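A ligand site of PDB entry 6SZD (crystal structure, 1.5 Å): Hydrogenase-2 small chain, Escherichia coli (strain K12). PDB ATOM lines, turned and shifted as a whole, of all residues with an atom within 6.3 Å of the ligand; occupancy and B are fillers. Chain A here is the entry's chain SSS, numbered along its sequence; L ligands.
The side-chain sulfur of Cys 225 sits close to the backbone NH of Cys 254. The side-chain sulfur (SG) of Cys 225 lies close to the backbone NH (N) of Gly 227 (3.4 Å). SG of Cys 219 lies close to N of Tyr 221 (3.3 Å). O of Trp 218 lies within hydrogen-bond range of NH1 of Arg 196 (2.9 Å). The backbone NH (N) of His 191 lies within hydrogen-bond range of the backbone carbonyl oxygen (O) of Gly 227 (3.2 Å). NH2 of Arg 196 is in hydrogen-bond range of O of Val 248, 3.2 Å away. The backbone carbonyl oxygen of Leu 220 is in hydrogen-bond range of the backbone NH of Cys 225 (3.3 Å). The backbone NH of Arg 196 lies close to the side-chain sulfur of Cys 194, at 3.3 Å.
FE1 of the ligand is bound by SG of Cys 219 (2.3 Å). N of Arg 197 sits close to S2 of the ligand. An iron atom (FE2) of the ligand is bound by the side-chain sulfur of Cys 225. The backbone NH (N) of Leu 220 lies close to a sulfur (S3) of the ligand (3.5 Å). FE3 of the ligand is bound by ND1 of His 191 (2.0 Å). An iron atom (FE4) of the ligand is bound by the side-chain sulfur (SG) of Cys 194 (2.3 Å).
A sulfur (S2) of the ligand sits close to the backbone carbonyl oxygen of Arg 196. CB of Phe 200 touches S2 of the ligand (3.9 Å). CB of Tyr 221 touches S4 of the ligand (3.6 Å). Gly 227 touches the ligand. CD of Pro 228 touches S4 of the ligand, 3.97 Å away. Val 248 touches the ligand (CG1 to S3, 3.9 Å). Of the 23 residues printed, 12 come within 4 Å of the ligand. Along chain A the residues within 4 Å of the ligand span positions 191 to 248. The nearest printed residue that does not touch the ligand is Ile 190 (4.1 Å).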
ATOM      1  N   ILE A 190     -30.793 -22.040   7.794  1.00  0.00           N
ATOM      2  CA  ILE A 190     -30.092 -21.998   6.490  1.00  0.00           C
ATOM      3  C   ILE A 190     -28.589 -21.852   6.711  1.00  0.00           C
ATOM      4  O   ILE A 190     -27.818 -22.587   6.069  1.00  0.00           O
ATOM      5  CB  ILE A 190     -30.701 -20.884   5.623  1.00  0.00           C
ATOM      6  CG1 ILE A 190     -32.120 -21.291   5.208  1.00  0.00           C
ATOM      7  CG2 ILE A 190     -29.798 -20.512   4.442  1.00  0.00           C
ATOM      8  CD1 ILE A 190     -32.941 -20.165   4.554  1.00  0.00           C
ATOM      9  N   HIS A 191     -28.176 -21.000   7.646  1.00  0.00           N
ATOM     10  CA  HIS A 191     -26.738 -20.736   7.903  1.00  0.00           C
ATOM     11  C   HIS A 191     -26.035 -21.957   8.504  1.00  0.00           C
ATOM     12  O   HIS A 191     -24.802 -22.000   8.395  1.00  0.00           O
ATOM     13  CB  HIS A 191     -26.635 -19.515   8.832  1.00  0.00           C
ATOM     14  CG  HIS A 191     -25.285 -19.094   9.243  1.00  0.00           C
ATOM     15  ND1 HIS A 191     -24.466 -18.350   8.443  1.00  0.00           N
ATOM     16  CD2 HIS A 191     -24.653 -19.279  10.437  1.00  0.00           C
ATOM     17  CE1 HIS A 191     -23.369 -18.064   9.156  1.00  0.00           C
ATOM     18  NE2 HIS A 191     -23.458 -18.630  10.372  1.00  0.00           N
ATOM     19  N   GLU A 192     -26.765 -22.901   9.081  1.00  0.00           N
ATOM     20  CA  GLU A 192     -26.172 -24.145   9.632  1.00  0.00           C
ATOM     21  C   GLU A 192     -26.156 -25.223   8.549  1.00  0.00           C
ATOM     22  O   GLU A 192     -25.787 -26.358   8.850  1.00  0.00           O
ATOM     23  CB  GLU A 192     -26.882 -24.578  10.901  1.00  0.00           C
ATOM     24  CG  GLU A 192     -26.657 -23.610  12.053  1.00  0.00           C
ATOM     25  CD  GLU A 192     -25.190 -23.445  12.409  1.00  0.00           C
ATOM     26  OE1 GLU A 192     -24.712 -22.292  12.464  1.00  0.00           O
ATOM     27  OE2 GLU A 192     -24.516 -24.456  12.581  1.00  0.00           O
ATOM     28  N   CYS A 194     -25.225 -23.937   4.920  1.00  0.00           N
ATOM     29  CA  CYS A 194     -24.991 -23.016   3.776  1.00  0.00           C
ATOM     30  C   CYS A 194     -23.596 -23.213   3.222  1.00  0.00           C
ATOM     31  O   CYS A 194     -22.604 -23.211   4.019  1.00  0.00           O
ATOM     32  CB  CYS A 194     -25.129 -21.549   4.196  1.00  0.00           C
ATOM     33  SG  CYS A 194     -24.804 -20.422   2.826  1.00  0.00           S
ATOM     34  N   GLU A 195     -23.473 -23.410   1.909  1.00  0.00           N
ATOM     35  CA  GLU A 195     -22.181 -23.672   1.245  1.00  0.00           C
ATOM     36  C   GLU A 195     -21.261 -22.461   1.330  1.00  0.00           C
ATOM     37  O   GLU A 195     -20.063 -22.602   1.001  1.00  0.00           O
ATOM     38  CB  GLU A 195     -22.413 -24.130  -0.183  1.00  0.00           C
ATOM     39  CG  GLU A 195     -22.985 -23.039  -1.099  1.00  0.00           C
ATOM     40  CD  GLU A 195     -24.511 -22.889  -1.176  1.00  0.00           C
ATOM     41  OE1 GLU A 195     -25.248 -23.426  -0.253  1.00  0.00           O
ATOM     42  OE2 GLU A 195     -24.971 -22.274  -2.221  1.00  0.00           O
ATOM     43  N   ARG A 196     -21.753 -21.293   1.786  1.00  0.00           N
ATOM     44  CA  ARG A 196     -20.868 -20.110   1.879  1.00  0.00           C
ATOM     45  C   ARG A 196     -20.337 -19.971   3.311  1.00  0.00           C
ATOM     46  O   ARG A 196     -19.583 -19.009   3.560  1.00  0.00           O
ATOM     47  CB  ARG A 196     -21.543 -18.835   1.386  1.00  0.00           C
ATOM     48  CG  ARG A 196     -21.917 -18.948  -0.098  1.00  0.00           C
ATOM     49  CD  ARG A 196     -22.314 -17.660  -0.718  1.00  0.00           C
ATOM     50  NE  ARG A 196     -22.591 -17.927  -2.130  1.00  0.00           N
ATOM     51  CZ  ARG A 196     -22.608 -17.021  -3.074  1.00  0.00           C
ATOM     52  NH1 ARG A 196     -22.384 -15.749  -2.802  1.00  0.00           N
ATOM     53  NH2 ARG A 196     -22.860 -17.393  -4.308  1.00  0.00           N
ATOM     54  N   ARG A 197     -20.671 -20.882   4.188  1.00  0.00           N
ATOM     55  CA  ARG A 197     -20.192 -20.843   5.581  1.00  0.00           C
ATOM     56  C   ARG A 197     -18.662 -20.739   5.596  1.00  0.00           C
ATOM     57  O   ARG A 197     -18.149 -20.025   6.483  1.00  0.00           O
ATOM     58  CB  ARG A 197     -20.705 -22.036   6.375  1.00  0.00           C
ATOM     59  CG  ARG A 197     -20.241 -21.997   7.826  1.00  0.00           C
ATOM     60  CD  ARG A 197     -20.724 -20.772   8.609  1.00  0.00           C
ATOM     61  NE  ARG A 197     -20.372 -21.003   9.994  1.00  0.00           N
ATOM     62  CZ  ARG A 197     -21.139 -21.588  10.906  1.00  0.00           C
ATOM     63  NH1 ARG A 197     -22.393 -21.906  10.665  1.00  0.00           N
ATOM     64  NH2 ARG A 197     -20.611 -21.860  12.085  1.00  0.00           N
ATOM     65  N   PRO A 198     -17.892 -21.441   4.744  1.00  0.00           N
ATOM     66  CA  PRO A 198     -16.420 -21.286   4.843  1.00  0.00           C
ATOM     67  C   PRO A 198     -15.976 -19.831   4.702  1.00  0.00           C
ATOM     68  O   PRO A 198     -14.961 -19.403   5.340  1.00  0.00           O
ATOM     69  CB  PRO A 198     -15.877 -22.136   3.693  1.00  0.00           C
ATOM     70  CG  PRO A 198     -16.955 -23.169   3.462  1.00  0.00           C
ATOM     71  CD  PRO A 198     -18.264 -22.424   3.719  1.00  0.00           C
ATOM     72  N   PHE A 200     -17.862 -17.071   5.359  1.00  0.00           N
ATOM     73  CA  PHE A 200     -18.253 -16.449   6.643  1.00  0.00           C
ATOM     74  C   PHE A 200     -17.138 -16.682   7.666  1.00  0.00           C
ATOM     75  O   PHE A 200     -16.693 -15.750   8.352  1.00  0.00           O
ATOM     76  CB  PHE A 200     -19.571 -17.033   7.131  1.00  0.00           C
ATOM     77  CG  PHE A 200     -20.050 -16.474   8.444  1.00  0.00           C
ATOM     78  CD1 PHE A 200     -19.662 -17.064   9.619  1.00  0.00           C
ATOM     79  CD2 PHE A 200     -20.954 -15.430   8.513  1.00  0.00           C
ATOM     80  CE1 PHE A 200     -20.103 -16.598  10.851  1.00  0.00           C
ATOM     81  CE2 PHE A 200     -21.403 -14.954   9.733  1.00  0.00           C
ATOM     82  CZ  PHE A 200     -21.000 -15.557  10.904  1.00  0.00           C
ATOM     83  N   PHE A 205     -16.252 -11.630   2.839  1.00  0.00           N
ATOM     84  CA  PHE A 205     -17.598 -11.037   2.703  1.00  0.00           C
ATOM     85  C   PHE A 205     -17.690 -10.190   1.445  1.00  0.00           C
ATOM     86  O   PHE A 205     -16.831  -9.368   1.167  1.00  0.00           O
ATOM     87  CB  PHE A 205     -17.935 -10.197   3.924  1.00  0.00           C
ATOM     88  CG  PHE A 205     -17.981 -10.965   5.215  1.00  0.00           C
ATOM     89  CD1 PHE A 205     -18.965 -11.908   5.457  1.00  0.00           C
ATOM     90  CD2 PHE A 205     -17.077 -10.671   6.256  1.00  0.00           C
ATOM     91  CE1 PHE A 205     -19.045 -12.583   6.653  1.00  0.00           C
ATOM     92  CE2 PHE A 205     -17.169 -11.374   7.446  1.00  0.00           C
ATOM     93  CZ  PHE A 205     -18.157 -12.317   7.666  1.00  0.00           C
ATOM     94  N   TRP A 218     -18.509 -15.058  -2.377  1.00  0.00           N
ATOM     95  CA  TRP A 218     -18.244 -14.999  -0.943  1.00  0.00           C
ATOM     96  C   TRP A 218     -19.534 -14.861  -0.142  1.00  0.00           C
ATOM     97  O   TRP A 218     -20.648 -14.667  -0.731  1.00  0.00           O
ATOM     98  CB  TRP A 218     -17.291 -13.837  -0.623  1.00  0.00           C
ATOM     99  CG  TRP A 218     -15.885 -14.088  -1.036  1.00  0.00           C
ATOM    100  CD1 TRP A 218     -15.371 -15.212  -1.635  1.00  0.00           C
ATOM    101  CD2 TRP A 218     -14.759 -13.213  -0.814  1.00  0.00           C
ATOM    102  NE1 TRP A 218     -14.034 -15.061  -1.849  1.00  0.00           N
ATOM    103  CE2 TRP A 218     -13.630 -13.853  -1.345  1.00  0.00           C
ATOM    104  CE3 TRP A 218     -14.605 -11.944  -0.230  1.00  0.00           C
ATOM    105  CZ2 TRP A 218     -12.354 -13.271  -1.317  1.00  0.00           C
ATOM    106  CZ3 TRP A 218     -13.348 -11.389  -0.179  1.00  0.00           C
ATOM    107  CH2 TRP A 218     -12.250 -12.047  -0.721  1.00  0.00           C
ATOM    108  N   CYS A 219     -19.398 -14.906   1.164  1.00  0.00           N
ATOM    109  CA  CYS A 219     -20.577 -14.864   2.066  1.00  0.00           C
ATOM    110  C   CYS A 219     -21.301 -13.517   1.940  1.00  0.00           C
ATOM    111  O   CYS A 219     -20.627 -12.481   1.748  1.00  0.00           O
ATOM    112  CB  CYS A 219     -20.171 -15.183   3.496  1.00  0.00           C
ATOM    113  SG  CYS A 219     -21.400 -14.839   4.777  1.00  0.00           S
ATOM    114  N   LEU A 220     -22.636 -13.551   2.066  1.00  0.00           N
ATOM    115  CA  LEU A 220     -23.525 -12.389   1.916  1.00  0.00           C
ATOM    116  C   LEU A 220     -23.953 -11.826   3.259  1.00  0.00           C
ATOM    117  O   LEU A 220     -24.880 -10.952   3.279  1.00  0.00           O
ATOM    118  CB  LEU A 220     -24.704 -12.752   0.988  1.00  0.00           C
ATOM    119  CG  LEU A 220     -24.297 -13.406  -0.341  1.00  0.00           C
ATOM    120  CD1 LEU A 220     -25.550 -13.538  -1.227  1.00  0.00           C
ATOM    121  CD2 LEU A 220     -23.250 -12.615  -1.070  1.00  0.00           C
ATOM    122  N   TYR A 221     -23.341 -12.215   4.367  1.00  0.00           N
ATOM    123  CA  TYR A 221     -23.722 -11.757   5.728  1.00  0.00           C
ATOM    124  C   TYR A 221     -23.792 -10.228   5.763  1.00  0.00           C
ATOM    125  O   TYR A 221     -24.815  -9.681   6.286  1.00  0.00           O
ATOM    126  CB  TYR A 221     -22.774 -12.309   6.812  1.00  0.00           C
ATOM    127  CG  TYR A 221     -23.174 -11.794   8.172  1.00  0.00           C
ATOM    128  CD1 TYR A 221     -24.303 -12.281   8.793  1.00  0.00           C
ATOM    129  CD2 TYR A 221     -22.467 -10.770   8.779  1.00  0.00           C
ATOM    130  CE1 TYR A 221     -24.737 -11.788  10.010  1.00  0.00           C
ATOM    131  CE2 TYR A 221     -22.912 -10.224   9.979  1.00  0.00           C
ATOM    132  CZ  TYR A 221     -24.052 -10.738  10.594  1.00  0.00           C
ATOM    133  OH  TYR A 221     -24.509 -10.219  11.788  1.00  0.00           O
ATOM    134  N   HIS A 222     -22.756  -9.557   5.288  1.00  0.00           N
ATOM    135  CA  HIS A 222     -22.689  -8.068   5.373  1.00  0.00           C
ATOM    136  C   HIS A 222     -23.547  -7.399   4.310  1.00  0.00           C
ATOM    137  O   HIS A 222     -23.610  -6.154   4.328  1.00  0.00           O
ATOM    138  CB  HIS A 222     -21.225  -7.569   5.367  1.00  0.00           C
ATOM    139  CG  HIS A 222     -20.639  -7.753   6.721  1.00  0.00           C
ATOM    140  ND1 HIS A 222     -20.922  -6.868   7.756  1.00  0.00           N
ATOM    141  CD2 HIS A 222     -19.822  -8.693   7.223  1.00  0.00           C
ATOM    142  CE1 HIS A 222     -20.301  -7.291   8.849  1.00  0.00           C
ATOM    143  NE2 HIS A 222     -19.610  -8.405   8.552  1.00  0.00           N
ATOM    144  N   CYS A 225     -27.753 -10.893   4.872  1.00  0.00           N
ATOM    145  CA  CYS A 225     -28.242 -12.296   4.770  1.00  0.00           C
ATOM    146  C   CYS A 225     -28.915 -12.698   6.090  1.00  0.00           C
ATOM    147  O   CYS A 225     -28.282 -12.606   7.176  1.00  0.00           O
ATOM    148  CB  CYS A 225     -27.139 -13.247   4.376  1.00  0.00           C
ATOM    149  SG  CYS A 225     -27.775 -14.919   4.093  1.00  0.00           S
ATOM    150  N   LYS A 226     -30.143 -13.198   6.024  1.00  0.00           N
ATOM    151  CA  LYS A 226     -30.896 -13.633   7.219  1.00  0.00           C
ATOM    152  C   LYS A 226     -30.764 -15.132   7.431  1.00  0.00           C
ATOM    153  O   LYS A 226     -31.454 -15.682   8.307  1.00  0.00           O
ATOM    154  CB  LYS A 226     -32.352 -13.224   7.052  1.00  0.00           C
ATOM    155  CG  LYS A 226     -32.557 -11.726   6.883  1.00  0.00           C
ATOM    156  CD  LYS A 226     -31.789 -10.887   7.903  1.00  0.00           C
ATOM    157  CE  LYS A 226     -32.196  -9.433   7.905  1.00  0.00           C
ATOM    158  NZ  LYS A 226     -31.945  -8.822   6.577  1.00  0.00           N
ATOM    159  N   GLY A 227     -29.916 -15.805   6.644  1.00  0.00           N
ATOM    160  CA  GLY A 227     -29.659 -17.251   6.848  1.00  0.00           C
ATOM    161  C   GLY A 227     -29.448 -17.593   8.337  1.00  0.00           C
ATOM    162  O   GLY A 227     -29.902 -18.632   8.833  1.00  0.00           O
ATOM    163  N   PRO A 228     -28.699 -16.761   9.101  1.00  0.00           N
ATOM    164  CA  PRO A 228     -28.450 -17.116  10.500  1.00  0.00           C
ATOM    165  C   PRO A 228     -29.669 -17.182  11.397  1.00  0.00           C
ATOM    166  O   PRO A 228     -29.561 -17.725  12.503  1.00  0.00           O
ATOM    167  CB  PRO A 228     -27.461 -16.036  10.946  1.00  0.00           C
ATOM    168  CG  PRO A 228     -26.768 -15.607   9.676  1.00  0.00           C
ATOM    169  CD  PRO A 228     -27.854 -15.670   8.603  1.00  0.00           C
ATOM    170  N   TRP A 246     -30.856 -20.865  -5.694  1.00  0.00           N
ATOM    171  CA  TRP A 246     -31.488 -20.252  -4.514  1.00  0.00           C
ATOM    172  C   TRP A 246     -30.961 -18.837  -4.402  1.00  0.00           C
ATOM    173  O   TRP A 246     -30.016 -18.479  -5.121  1.00  0.00           O
ATOM    174  CB  TRP A 246     -31.302 -21.072  -3.235  1.00  0.00           C
ATOM    175  CG  TRP A 246     -29.925 -21.147  -2.638  1.00  0.00           C
ATOM    176  CD1 TRP A 246     -28.820 -21.784  -3.095  1.00  0.00           C
ATOM    177  CD2 TRP A 246     -29.586 -20.658  -1.333  1.00  0.00           C
ATOM    178  NE1 TRP A 246     -27.807 -21.724  -2.176  1.00  0.00           N
ATOM    179  CE2 TRP A 246     -28.240 -21.030  -1.070  1.00  0.00           C
ATOM    180  CE3 TRP A 246     -30.276 -19.920  -0.370  1.00  0.00           C
ATOM    181  CZ2 TRP A 246     -27.620 -20.709   0.159  1.00  0.00           C
ATOM    182  CZ3 TRP A 246     -29.696 -19.656   0.845  1.00  0.00           C
ATOM    183  CH2 TRP A 246     -28.373 -20.053   1.094  1.00  0.00           C
ATOM    184  N   VAL A 248     -29.154 -16.935  -2.416  1.00  0.00           N
ATOM    185  CA  VAL A 248     -27.718 -16.708  -2.081  1.00  0.00           C
ATOM    186  C   VAL A 248     -26.857 -17.217  -3.228  1.00  0.00           C
ATOM    187  O   VAL A 248     -25.903 -16.519  -3.631  1.00  0.00           O
ATOM    188  CB  VAL A 248     -27.381 -17.423  -0.762  1.00  0.00           C
ATOM    189  CG1 VAL A 248     -25.876 -17.557  -0.594  1.00  0.00           C
ATOM    190  CG2 VAL A 248     -28.032 -16.667   0.380  1.00  0.00           C
ATOM    191  N   PRO A 253     -28.675 -11.889  -0.676  1.00  0.00           N
ATOM    192  CA  PRO A 253     -28.869 -12.422   0.671  1.00  0.00           C
ATOM    193  C   PRO A 253     -30.270 -13.025   0.834  1.00  0.00           C
ATOM    194  O   PRO A 253     -31.227 -12.577   0.205  1.00  0.00           O
ATOM    195  CB  PRO A 253     -28.657 -11.174   1.563  1.00  0.00           C
ATOM    196  CG  PRO A 253     -28.917 -10.006   0.682  1.00  0.00           C
ATOM    197  CD  PRO A 253     -28.361 -10.455  -0.648  1.00  0.00           C
ATOM    198  N   CYS A 254     -30.356 -14.031   1.696  1.00  0.00           N
ATOM    199  CA  CYS A 254     -31.647 -14.450   2.282  1.00  0.00           C
ATOM    200  C   CYS A 254     -32.267 -13.223   2.971  1.00  0.00           C
ATOM    201  O   CYS A 254     -31.555 -12.439   3.628  1.00  0.00           O
ATOM    202  CB  CYS A 254     -31.453 -15.631   3.219  1.00  0.00           C
ATOM    203  SG  CYS A 254     -32.943 -16.139   4.118  1.00  0.00           S
HETATM  204 FE1  LIG L   1     -23.162 -16.298   4.739  1.00  0.00          FE
HETATM  205 FE2  LIG L   1     -25.915 -16.209   4.578  1.00  0.00          FE
HETATM  206 FE3  LIG L   1     -24.680 -17.664   6.550  1.00  0.00          FE
HETATM  207 FE4  LIG L   1     -24.613 -18.481   3.973  1.00  0.00          FE
HETATM  208  S1  LIG L   1     -26.503 -18.272   5.321  1.00  0.00           S
HETATM  209  S2  LIG L   1     -22.815 -18.434   5.408  1.00  0.00           S
HETATM  210  S3  LIG L   1     -24.421 -16.510   2.858  1.00  0.00           S
HETATM  211  S4  LIG L   1     -24.630 -15.398   6.299  1.00  0.00           S
